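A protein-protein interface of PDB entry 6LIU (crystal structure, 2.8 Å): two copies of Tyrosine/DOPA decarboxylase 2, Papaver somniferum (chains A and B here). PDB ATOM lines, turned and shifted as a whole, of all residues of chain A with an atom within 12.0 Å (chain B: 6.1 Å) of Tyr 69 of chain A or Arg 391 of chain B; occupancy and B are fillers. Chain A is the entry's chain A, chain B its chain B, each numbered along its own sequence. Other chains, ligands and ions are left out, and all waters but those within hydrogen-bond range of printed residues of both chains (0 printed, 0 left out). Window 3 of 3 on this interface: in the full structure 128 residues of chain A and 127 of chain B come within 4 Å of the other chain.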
ATOM      1  N   THR A  19       0.697  20.372 -19.821  1.00  0.00           N
ATOM      2  CA  THR A  19       0.806  19.839 -21.176  1.00  0.00           C
ATOM      3  C   THR A  19      -0.559  19.405 -21.697  1.00  0.00           C
ATOM      4  O   THR A  19      -1.306  18.714 -21.003  1.00  0.00           O
ATOM      5  CB  THR A  19       1.774  18.645 -21.239  1.00  0.00           C
ATOM      6  OG1 THR A  19       2.849  18.853 -20.317  1.00  0.00           O
ATOM      7  CG2 THR A  19       2.334  18.484 -22.648  1.00  0.00           C
ATOM      8  N   PRO A  21      -3.536  17.472 -23.319  1.00  0.00           N
ATOM      9  CA  PRO A  21      -3.762  16.028 -23.493  1.00  0.00           C
ATOM     10  C   PRO A  21      -3.783  15.582 -24.944  1.00  0.00           C
ATOM     11  O   PRO A  21      -3.771  14.371 -25.197  1.00  0.00           O
ATOM     12  CB  PRO A  21      -5.125  15.798 -22.827  1.00  0.00           C
ATOM     13  CG  PRO A  21      -5.384  17.023 -22.004  1.00  0.00           C
ATOM     14  CD  PRO A  21      -4.685  18.143 -22.693  1.00  0.00           C
ATOM     15  N   PRO A  64      -5.402  -1.585  -8.088  1.00  0.00           N
ATOM     16  CA  PRO A  64      -5.931  -0.834  -6.943  1.00  0.00           C
ATOM     17  C   PRO A  64      -7.433  -0.616  -7.066  1.00  0.00           C
ATOM     18  O   PRO A  64      -8.052  -0.865  -8.102  1.00  0.00           O
ATOM     19  CB  PRO A  64      -5.160   0.490  -6.986  1.00  0.00           C
ATOM     20  CG  PRO A  64      -4.558   0.558  -8.360  1.00  0.00           C
ATOM     21  CD  PRO A  64      -4.347  -0.846  -8.803  1.00  0.00           C
ATOM     22  N   GLU A  65      -8.021  -0.143  -5.967  1.00  0.00           N
ATOM     23  CA  GLU A  65      -9.463   0.041  -5.876  1.00  0.00           C
ATOM     24  C   GLU A  65      -9.924   1.447  -6.239  1.00  0.00           C
ATOM     25  O   GLU A  65     -11.135   1.675  -6.334  1.00  0.00           O
ATOM     26  CB  GLU A  65      -9.954  -0.283  -4.463  1.00  0.00           C
ATOM     27  CG  GLU A  65      -9.403  -1.565  -3.882  1.00  0.00           C
ATOM     28  CD  GLU A  65     -10.175  -2.011  -2.657  1.00  0.00           C
ATOM     29  OE1 GLU A  65      -9.537  -2.382  -1.650  1.00  0.00           O
ATOM     30  OE2 GLU A  65     -11.424  -1.983  -2.703  1.00  0.00           O
ATOM     31  N   THR A  66      -9.004   2.390  -6.423  1.00  0.00           N
ATOM     32  CA  THR A  66      -9.350   3.760  -6.763  1.00  0.00           C
ATOM     33  C   THR A  66      -8.470   4.235  -7.908  1.00  0.00           C
ATOM     34  O   THR A  66      -7.423   3.653  -8.198  1.00  0.00           O
ATOM     35  CB  THR A  66      -9.193   4.712  -5.563  1.00  0.00           C
ATOM     36  OG1 THR A  66      -7.837   4.688  -5.099  1.00  0.00           O
ATOM     37  CG2 THR A  66     -10.123   4.312  -4.429  1.00  0.00           C
ATOM     38  N   ALA A  67      -8.914   5.300  -8.564  1.00  0.00           N
ATOM     39  CA  ALA A  67      -8.108   5.910  -9.603  1.00  0.00           C
ATOM     40  C   ALA A  67      -6.913   6.626  -8.978  1.00  0.00           C
ATOM     41  O   ALA A  67      -6.985   7.088  -7.838  1.00  0.00           O
ATOM     42  CB  ALA A  67      -8.941   6.898 -10.414  1.00  0.00           C
ATOM     43  N   PRO A  68      -5.798   6.725  -9.698  1.00  0.00           N
ATOM     44  CA  PRO A  68      -4.665   7.498  -9.179  1.00  0.00           C
ATOM     45  C   PRO A  68      -4.963   8.987  -9.213  1.00  0.00           C
ATOM     46  O   PRO A  68      -5.496   9.510 -10.194  1.00  0.00           O
ATOM     47  CB  PRO A  68      -3.519   7.136 -10.131  1.00  0.00           C
ATOM     48  CG  PRO A  68      -4.202   6.773 -11.410  1.00  0.00           C
ATOM     49  CD  PRO A  68      -5.511   6.129 -11.016  1.00  0.00           C
ATOM     50  N   TYR A  69      -4.614   9.674  -8.123  1.00  0.00           N
ATOM     51  CA  TYR A  69      -4.758  11.126  -8.106  1.00  0.00           C
ATOM     52  C   TYR A  69      -3.739  11.799  -9.013  1.00  0.00           C
ATOM     53  O   TYR A  69      -3.996  12.891  -9.531  1.00  0.00           O
ATOM     54  CB  TYR A  69      -4.626  11.658  -6.676  1.00  0.00           C
ATOM     55  CG  TYR A  69      -5.925  11.641  -5.900  1.00  0.00           C
ATOM     56  CD1 TYR A  69      -6.896  12.614  -6.110  1.00  0.00           C
ATOM     57  CD2 TYR A  69      -6.183  10.651  -4.961  1.00  0.00           C
ATOM     58  CE1 TYR A  69      -8.087  12.602  -5.403  1.00  0.00           C
ATOM     59  CE2 TYR A  69      -7.371  10.631  -4.251  1.00  0.00           C
ATOM     60  CZ  TYR A  69      -8.318  11.608  -4.475  1.00  0.00           C
ATOM     61  OH  TYR A  69      -9.501  11.585  -3.769  1.00  0.00           O
ATOM     62  N   ASN A  70      -2.594  11.160  -9.234  1.00  0.00           N
ATOM     63  CA  ASN A  70      -1.513  11.766  -9.990  1.00  0.00           C
ATOM     64  C   ASN A  70      -1.209  10.963 -11.250  1.00  0.00           C
ATOM     65  O   ASN A  70      -1.466   9.756 -11.300  1.00  0.00           O
ATOM     66  CB  ASN A  70      -0.255  11.873  -9.120  1.00  0.00           C
ATOM     67  CG  ASN A  70      -0.491  12.702  -7.880  1.00  0.00           C
ATOM     68  OD1 ASN A  70      -0.975  13.832  -7.959  1.00  0.00           O
ATOM     69  ND2 ASN A  70      -0.168  12.142  -6.721  1.00  0.00           N
ATOM     70  N   PRO A  71      -0.670  11.603 -12.285  1.00  0.00           N
ATOM     71  CA  PRO A  71      -0.434  10.891 -13.546  1.00  0.00           C
ATOM     72  C   PRO A  71       0.612   9.796 -13.404  1.00  0.00           C
ATOM     73  O   PRO A  71       1.484   9.837 -12.533  1.00  0.00           O
ATOM     74  CB  PRO A  71       0.051  11.996 -14.493  1.00  0.00           C
ATOM     75  CG  PRO A  71       0.587  13.061 -13.593  1.00  0.00           C
ATOM     76  CD  PRO A  71      -0.279  13.022 -12.369  1.00  0.00           C
ATOM     77  N   GLU A  72       0.503   8.803 -14.279  1.00  0.00           N
ATOM     78  CA  GLU A  72       1.494   7.747 -14.413  1.00  0.00           C
ATOM     79  C   GLU A  72       2.036   7.765 -15.834  1.00  0.00           C
ATOM     80  O   GLU A  72       1.344   8.172 -16.771  1.00  0.00           O
ATOM     81  CB  GLU A  72       0.898   6.369 -14.088  1.00  0.00           C
ATOM     82  CG  GLU A  72      -0.025   6.356 -12.875  1.00  0.00           C
ATOM     83  CD  GLU A  72      -0.304   4.951 -12.370  1.00  0.00           C
ATOM     84  OE1 GLU A  72       0.625   4.325 -11.816  1.00  0.00           O
ATOM     85  OE2 GLU A  72      -1.449   4.473 -12.524  1.00  0.00           O
ATOM     86  N   SER A  73       3.281   7.327 -15.988  1.00  0.00           N
ATOM     87  CA  SER A  73       3.939   7.399 -17.283  1.00  0.00           C
ATOM     88  C   SER A  73       3.442   6.294 -18.208  1.00  0.00           C
ATOM     89  O   SER A  73       3.000   5.230 -17.763  1.00  0.00           O
ATOM     90  CB  SER A  73       5.455   7.300 -17.125  1.00  0.00           C
ATOM     91  OG  SER A  73       5.856   5.962 -16.888  1.00  0.00           O
ATOM     92  N   ILE A  77       2.576   2.290 -17.684  1.00  0.00           N
ATOM     93  CA  ILE A  77       1.296   1.718 -18.090  1.00  0.00           C
ATOM     94  C   ILE A  77       1.510   0.553 -19.051  1.00  0.00           C
ATOM     95  O   ILE A  77       0.868  -0.498 -18.931  1.00  0.00           O
ATOM     96  CB  ILE A  77       0.403   2.813 -18.705  1.00  0.00           C
ATOM     97  CG1 ILE A  77       0.044   3.866 -17.654  1.00  0.00           C
ATOM     98  CG2 ILE A  77      -0.857   2.212 -19.297  1.00  0.00           C
ATOM     99  CD1 ILE A  77      -0.558   5.137 -18.231  1.00  0.00           C
ATOM    100  N   MET B 146     -15.109   8.305  -8.441  1.00  0.00           N
ATOM    101  CA  MET B 146     -14.728   9.680  -8.741  1.00  0.00           C
ATOM    102  C   MET B 146     -15.949  10.585  -8.841  1.00  0.00           C
ATOM    103  O   MET B 146     -15.871  11.777  -8.520  1.00  0.00           O
ATOM    104  CB  MET B 146     -13.923   9.732 -10.040  1.00  0.00           C
ATOM    105  CG  MET B 146     -12.524   9.157  -9.934  1.00  0.00           C
ATOM    106  SD  MET B 146     -11.774   8.886 -11.554  1.00  0.00           S
ATOM    107  CE  MET B 146     -11.703  10.559 -12.196  1.00  0.00           C
ATOM    108  N   ILE B 296     -16.963  14.929 -11.225  1.00  0.00           N
ATOM    109  CA  ILE B 296     -15.820  14.431 -10.466  1.00  0.00           C
ATOM    110  C   ILE B 296     -15.157  15.551  -9.674  1.00  0.00           C
ATOM    111  O   ILE B 296     -14.406  15.273  -8.735  1.00  0.00           O
ATOM    112  CB  ILE B 296     -14.773  13.750 -11.365  1.00  0.00           C
ATOM    113  CG1 ILE B 296     -14.111  14.764 -12.298  1.00  0.00           C
ATOM    114  CG2 ILE B 296     -15.396  12.607 -12.154  1.00  0.00           C
ATOM    115  CD1 ILE B 296     -12.874  14.229 -12.978  1.00  0.00           C
ATOM    116  N   CYS B 297     -15.410  16.811 -10.037  1.00  0.00           N
ATOM    117  CA  CYS B 297     -14.989  17.956  -9.236  1.00  0.00           C
ATOM    118  C   CYS B 297     -16.033  18.229  -8.158  1.00  0.00           C
ATOM    119  O   CYS B 297     -17.221  18.332  -8.475  1.00  0.00           O
ATOM    120  CB  CYS B 297     -14.823  19.198 -10.107  1.00  0.00           C
ATOM    121  SG  CYS B 297     -14.137  18.912 -11.746  1.00  0.00           S
ATOM    122  N   PRO B 298     -15.637  18.364  -6.889  1.00  0.00           N
ATOM    123  CA  PRO B 298     -16.644  18.543  -5.826  1.00  0.00           C
ATOM    124  C   PRO B 298     -17.571  19.729  -6.041  1.00  0.00           C
ATOM    125  O   PRO B 298     -18.731  19.666  -5.619  1.00  0.00           O
ATOM    126  CB  PRO B 298     -15.783  18.717  -4.567  1.00  0.00           C
ATOM    127  CG  PRO B 298     -14.523  17.999  -4.872  1.00  0.00           C
ATOM    128  CD  PRO B 298     -14.274  18.242  -6.342  1.00  0.00           C
ATOM    129  N   GLU B 299     -17.115  20.797  -6.699  1.00  0.00           N
ATOM    130  CA  GLU B 299     -17.966  21.973  -6.864  1.00  0.00           C
ATOM    131  C   GLU B 299     -19.109  21.759  -7.854  1.00  0.00           C
ATOM    132  O   GLU B 299     -20.036  22.576  -7.875  1.00  0.00           O
ATOM    133  CB  GLU B 299     -17.130  23.184  -7.292  1.00  0.00           C
ATOM    134  CG  GLU B 299     -16.523  23.082  -8.673  1.00  0.00           C
ATOM    135  CD  GLU B 299     -15.104  22.542  -8.649  1.00  0.00           C
ATOM    136  OE1 GLU B 299     -14.775  21.754  -7.733  1.00  0.00           O
ATOM    137  OE2 GLU B 299     -14.320  22.900  -9.553  1.00  0.00           O
ATOM    138  N   TYR B 385      -3.420  10.610 -16.899  1.00  0.00           N
ATOM    139  CA  TYR B 385      -3.654  11.956 -16.385  1.00  0.00           C
ATOM    140  C   TYR B 385      -3.990  11.994 -14.903  1.00  0.00           C
ATOM    141  O   TYR B 385      -3.573  12.924 -14.209  1.00  0.00           O
ATOM    142  CB  TYR B 385      -4.769  12.639 -17.186  1.00  0.00           C
ATOM    143  CG  TYR B 385      -4.545  12.539 -18.676  1.00  0.00           C
ATOM    144  CD1 TYR B 385      -3.379  13.019 -19.254  1.00  0.00           C
ATOM    145  CD2 TYR B 385      -5.489  11.944 -19.501  1.00  0.00           C
ATOM    146  CE1 TYR B 385      -3.163  12.920 -20.618  1.00  0.00           C
ATOM    147  CE2 TYR B 385      -5.282  11.839 -20.866  1.00  0.00           C
ATOM    148  CZ  TYR B 385      -4.119  12.327 -21.419  1.00  0.00           C
ATOM    149  OH  TYR B 385      -3.912  12.219 -22.778  1.00  0.00           O
ATOM    150  N   GLY B 386      -4.725  11.009 -14.393  1.00  0.00           N
ATOM    151  CA  GLY B 386      -5.053  10.991 -12.981  1.00  0.00           C
ATOM    152  C   GLY B 386      -6.123  11.991 -12.584  1.00  0.00           C
ATOM    153  O   GLY B 386      -6.414  12.935 -13.325  1.00  0.00           O
ATOM    154  N   VAL B 387      -6.691  11.803 -11.391  1.00  0.00           N
ATOM    155  CA  VAL B 387      -7.897  12.534 -11.007  1.00  0.00           C
ATOM    156  C   VAL B 387      -7.642  14.039 -10.985  1.00  0.00           C
ATOM    157  O   VAL B 387      -8.425  14.824 -11.532  1.00  0.00           O
ATOM    158  CB  VAL B 387      -8.414  12.026  -9.650  1.00  0.00           C
ATOM    159  CG1 VAL B 387      -9.449  12.988  -9.071  1.00  0.00           C
ATOM    160  CG2 VAL B 387      -8.988  10.626  -9.808  1.00  0.00           C
ATOM    161  N   THR B 388      -6.540  14.462 -10.358  1.00  0.00           N
ATOM    162  CA  THR B 388      -6.282  15.890 -10.183  1.00  0.00           C
ATOM    163  C   THR B 388      -6.213  16.613 -11.524  1.00  0.00           C
ATOM    164  O   THR B 388      -6.864  17.647 -11.720  1.00  0.00           O
ATOM    165  CB  THR B 388      -4.985  16.097  -9.399  1.00  0.00           C
ATOM    166  OG1 THR B 388      -5.061  15.409  -8.144  1.00  0.00           O
ATOM    167  CG2 THR B 388      -4.745  17.584  -9.146  1.00  0.00           C
ATOM    168  N   ASN B 389      -5.425  16.081 -12.464  1.00  0.00           N
ATOM    169  CA  ASN B 389      -5.309  16.711 -13.775  1.00  0.00           C
ATOM    170  C   ASN B 389      -6.649  16.732 -14.497  1.00  0.00           C
ATOM    171  O   ASN B 389      -6.994  17.720 -15.157  1.00  0.00           O
ATOM    172  CB  ASN B 389      -4.272  15.977 -14.622  1.00  0.00           C
ATOM    173  CG  ASN B 389      -2.855  16.418 -14.322  1.00  0.00           C
ATOM    174  OD1 ASN B 389      -2.617  17.553 -13.902  1.00  0.00           O
ATOM    175  ND2 ASN B 389      -1.899  15.520 -14.545  1.00  0.00           N
ATOM    176  N   LEU B 390      -7.415  15.643 -14.389  1.00  0.00           N
ATOM    177  CA  LEU B 390      -8.689  15.561 -15.091  1.00  0.00           C
ATOM    178  C   LEU B 390      -9.666  16.614 -14.587  1.00  0.00           C
ATOM    179  O   LEU B 390     -10.334  17.282 -15.387  1.00  0.00           O
ATOM    180  CB  LEU B 390      -9.273  14.159 -14.943  1.00  0.00           C
ATOM    181  CG  LEU B 390      -8.502  13.087 -15.710  1.00  0.00           C
ATOM    182  CD1 LEU B 390      -8.824  11.707 -15.167  1.00  0.00           C
ATOM    183  CD2 LEU B 390      -8.795  13.172 -17.197  1.00  0.00           C
ATOM    184  N   ARG B 391      -9.762  16.777 -13.265  1.00  0.00           N
ATOM    185  CA  ARG B 391     -10.629  17.811 -12.707  1.00  0.00           C
ATOM    186  C   ARG B 391     -10.265  19.185 -13.254  1.00  0.00           C
ATOM    187  O   ARG B 391     -11.145  20.010 -13.524  1.00  0.00           O
ATOM    188  CB  ARG B 391     -10.536  17.810 -11.180  1.00  0.00           C
ATOM    189  CG  ARG B 391     -11.141  16.593 -10.503  1.00  0.00           C
ATOM    190  CD  ARG B 391     -10.742  16.532  -9.039  1.00  0.00           C
ATOM    191  NE  ARG B 391     -11.684  15.750  -8.247  1.00  0.00           N
ATOM    192  CZ  ARG B 391     -11.450  15.321  -7.011  1.00  0.00           C
ATOM    193  NH1 ARG B 391     -10.297  15.596  -6.421  1.00  0.00           N
ATOM    194  NH2 ARG B 391     -12.371  14.618  -6.367  1.00  0.00           N
ATOM    195  N   ASN B 392      -8.970  19.444 -13.432  1.00  0.00           N
ATOM    196  CA  ASN B 392      -8.546  20.761 -13.884  1.00  0.00           C
ATOM    197  C   ASN B 392      -8.704  20.923 -15.389  1.00  0.00           C
ATOM    198  O   ASN B 392      -8.946  22.039 -15.864  1.00  0.00           O
ATOM    199  CB  ASN B 392      -7.106  21.018 -13.442  1.00  0.00           C
ATOM    200  CG  ASN B 392      -6.971  21.085 -11.925  1.00  0.00           C
ATOM    201  OD1 ASN B 392      -7.608  21.912 -11.268  1.00  0.00           O
ATOM    202  ND2 ASN B 392      -6.149  20.208 -11.364  1.00  0.00           N
ATOM    203  N   PHE B 393      -8.582  19.832 -16.149  1.00  0.00           N
ATOM    204  CA  PHE B 393      -8.959  19.872 -17.558  1.00  0.00           C
ATOM    205  C   PHE B 393     -10.399  20.346 -17.712  1.00  0.00           C
ATOM    206  O   PHE B 393     -10.683  21.290 -18.461  1.00  0.00           O
ATOM    207  CB  PHE B 393      -8.792  18.494 -18.194  1.00  0.00           C
ATOM    208  CG  PHE B 393      -7.374  18.037 -18.314  1.00  0.00           C
ATOM    209  CD1 PHE B 393      -6.324  18.930 -18.201  1.00  0.00           C
ATOM    210  CD2 PHE B 393      -7.091  16.701 -18.550  1.00  0.00           C
ATOM    211  CE1 PHE B 393      -5.014  18.500 -18.315  1.00  0.00           C
ATOM    212  CE2 PHE B 393      -5.785  16.263 -18.660  1.00  0.00           C
ATOM    213  CZ  PHE B 393      -4.745  17.165 -18.543  1.00  0.00           C
ATOM    214  N   LEU B 394     -11.327  19.694 -17.003  1.00  0.00           N
ATOM    215  CA  LEU B 394     -12.720  20.116 -17.047  1.00  0.00           C
ATOM    216  C   LEU B 394     -12.874  21.533 -16.514  1.00  0.00           C
ATOM    217  O   LEU B 394     -13.649  22.330 -17.059  1.00  0.00           O
ATOM    218  CB  LEU B 394     -13.592  19.138 -16.257  1.00  0.00           C
ATOM    219  CG  LEU B 394     -13.437  17.658 -16.633  1.00  0.00           C
ATOM    220  CD1 LEU B 394     -14.244  16.763 -15.706  1.00  0.00           C
ATOM    221  CD2 LEU B 394     -13.818  17.405 -18.086  1.00  0.00           C
ATOM    222  N   ARG B 395     -12.123  21.874 -15.464  1.00  0.00           N
ATOM    223  CA  ARG B 395     -12.221  23.215 -14.895  1.00  0.00           C
ATOM    224  C   ARG B 395     -11.748  24.277 -15.880  1.00  0.00           C
ATOM    225  O   ARG B 395     -12.310  25.377 -15.929  1.00  0.00           O
ATOM    226  CB  ARG B 395     -11.425  23.294 -13.598  1.00  0.00           C
ATOM    227  CG  ARG B 395     -12.222  22.893 -12.373  1.00  0.00           C
ATOM    228  CD  ARG B 395     -11.320  22.469 -11.225  1.00  0.00           C
ATOM    229  NE  ARG B 395     -12.108  21.987 -10.098  1.00  0.00           N
ATOM    230  CZ  ARG B 395     -11.623  21.256  -9.102  1.00  0.00           C
ATOM    231  NH1 ARG B 395     -10.337  20.921  -9.088  1.00  0.00           N
ATOM    232  NH2 ARG B 395     -12.425  20.859  -8.125  1.00  0.00           N
ATOM    233  N   SER B 396     -10.724  23.967 -16.677  1.00  0.00           N
ATOM    234  CA  SER B 396     -10.223  24.951 -17.632  1.00  0.00           C
ATOM    235  C   SER B 396     -11.269  25.280 -18.691  1.00  0.00           C
ATOM    236  O   SER B 396     -11.438  26.450 -19.057  1.00  0.00           O
ATOM    237  CB  SER B 396      -8.935  24.449 -18.283  1.00  0.00           C
ATOM    238  OG  SER B 396      -9.094  23.126 -18.758  1.00  0.00           O
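O of Pro 21 of chain A sits at hydrogen-bond distance from OH of Tyr 385 of chain B. N of Val 387 of chain B lies within hydrogen-bond range of O of Pro 68 of chain A. The backbone carbonyl oxygen (O) of Tyr 69 of chain A sits at hydrogen-bond distance from the backbone NH (N) of Val 387 of chain B (3.5 Å). O of Tyr 69 of chain A sits at hydrogen-bond distance from OG1 of Thr 388 of chain B (3.1 Å).
The backbone carbonyl oxygen (O) of Ile 296 of chain B lies within hydrogen-bond range of the guanidinium group (NE) of Arg 391 of chain B. The side-chain sulfur of Cys 297 of chain B sits at hydrogen-bond distance from the backbone carbonyl oxygen of Arg 391 of chain B. ND2 of Asn 389 of chain B sits at hydrogen-bond distance from O of Tyr 385 of chain B. The backbone carbonyl oxygen of Thr 388 of chain B is in hydrogen-bond range of the side-chain amide nitrogen of Asn 392 of chain B, at 2.7 Å. OG of Ser 396 of chain B sits at hydrogen-bond distance from O of Phe 393 of chain B (2.4 Å).
Among the printed residues, merely in contact across the chains: Pro 21 of chain A with Phe 393 of chain B (3.5 Å), Ala 67 of chain A with Met 146 of chain B (3.6 Å), Ala 67 of chain A with Val 387 of chain B (3.8 Å), Pro 68 of chain A with Gly 386 of chain B (3.2 Å), Tyr 69 of chain A with Gly 386 of chain B (3.8 Å), Tyr 69 of chain A with Arg 391 of chain B (3.9 Å), Pro 71 of chain A with Tyr 385 of chain B (3.7 Å) and Pro 71 of chain A with Asn 389 of chain B (3.6 Å).
Tyr 69 of chain A touches just these residues of chain B: Gly 386, Val 387, Thr 388 and Arg 391. Arg 391 of chain B touches one residue of chain A. Of chain A, only Ala 67 comes within 4 Å of Met 146 of chain B. Ile 296 of chain B touches none of the printed residues of chain A. No residue of chain A comes within 4 Å of Cys 297 of chain B. Of chain A, only Ala 67, Pro 68 and Tyr 69 come within 4 Å of Val 387 of chain B. Thr 388 of chain B touches just one residue of chain A: Tyr 69 (3.1 Å). Asn 389 of chain B touches just one residue of chain A: Pro 71. No residue of chain A comes within 4 Å of Leu 390 of chain B. Printed residues of chain A within 4 Å of Phe 393 of chain B: Pro 21 (3.5 Å). No residue of chain A comes within 4 Å of Leu 394 of chain B. Printed residues of chain A within 4 Å of Tyr 385 of chain B: Pro 21 and Pro 71. Of the printed residues of chain B, Pro 71 of chain A touches Tyr 385 and Asn 389. Pro 298 of chain B touches none of the printed residues of chain A.
Of the 17 printed residues of chain B, 8 touch a printed residue of chain A. Hydrophobic or aromatic side chains of chain B that line the printed part of chain A: Met 146, Tyr 385, Val 387 and Phe 393. Of the 13 printed residues of chain A, 5 touch a printed residue of chain B. Printed residues of chain A that touch a printed residue of chain B: Pro 21, Ala 67, Pro 68, Tyr 69 and Pro 71. Hydrophobic or aromatic side chains of chain A that line the printed part of chain B: Pro 21, Ala 67, Tyr 69 and Pro 71. Among the printed residues, 12 pairs touch across the chains. Among the printed residues, no Asp or Glu carboxylate lies within 4 Å of a Lys or Arg side-chain nitrogen of the other chain.
No position is printed for both chains.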
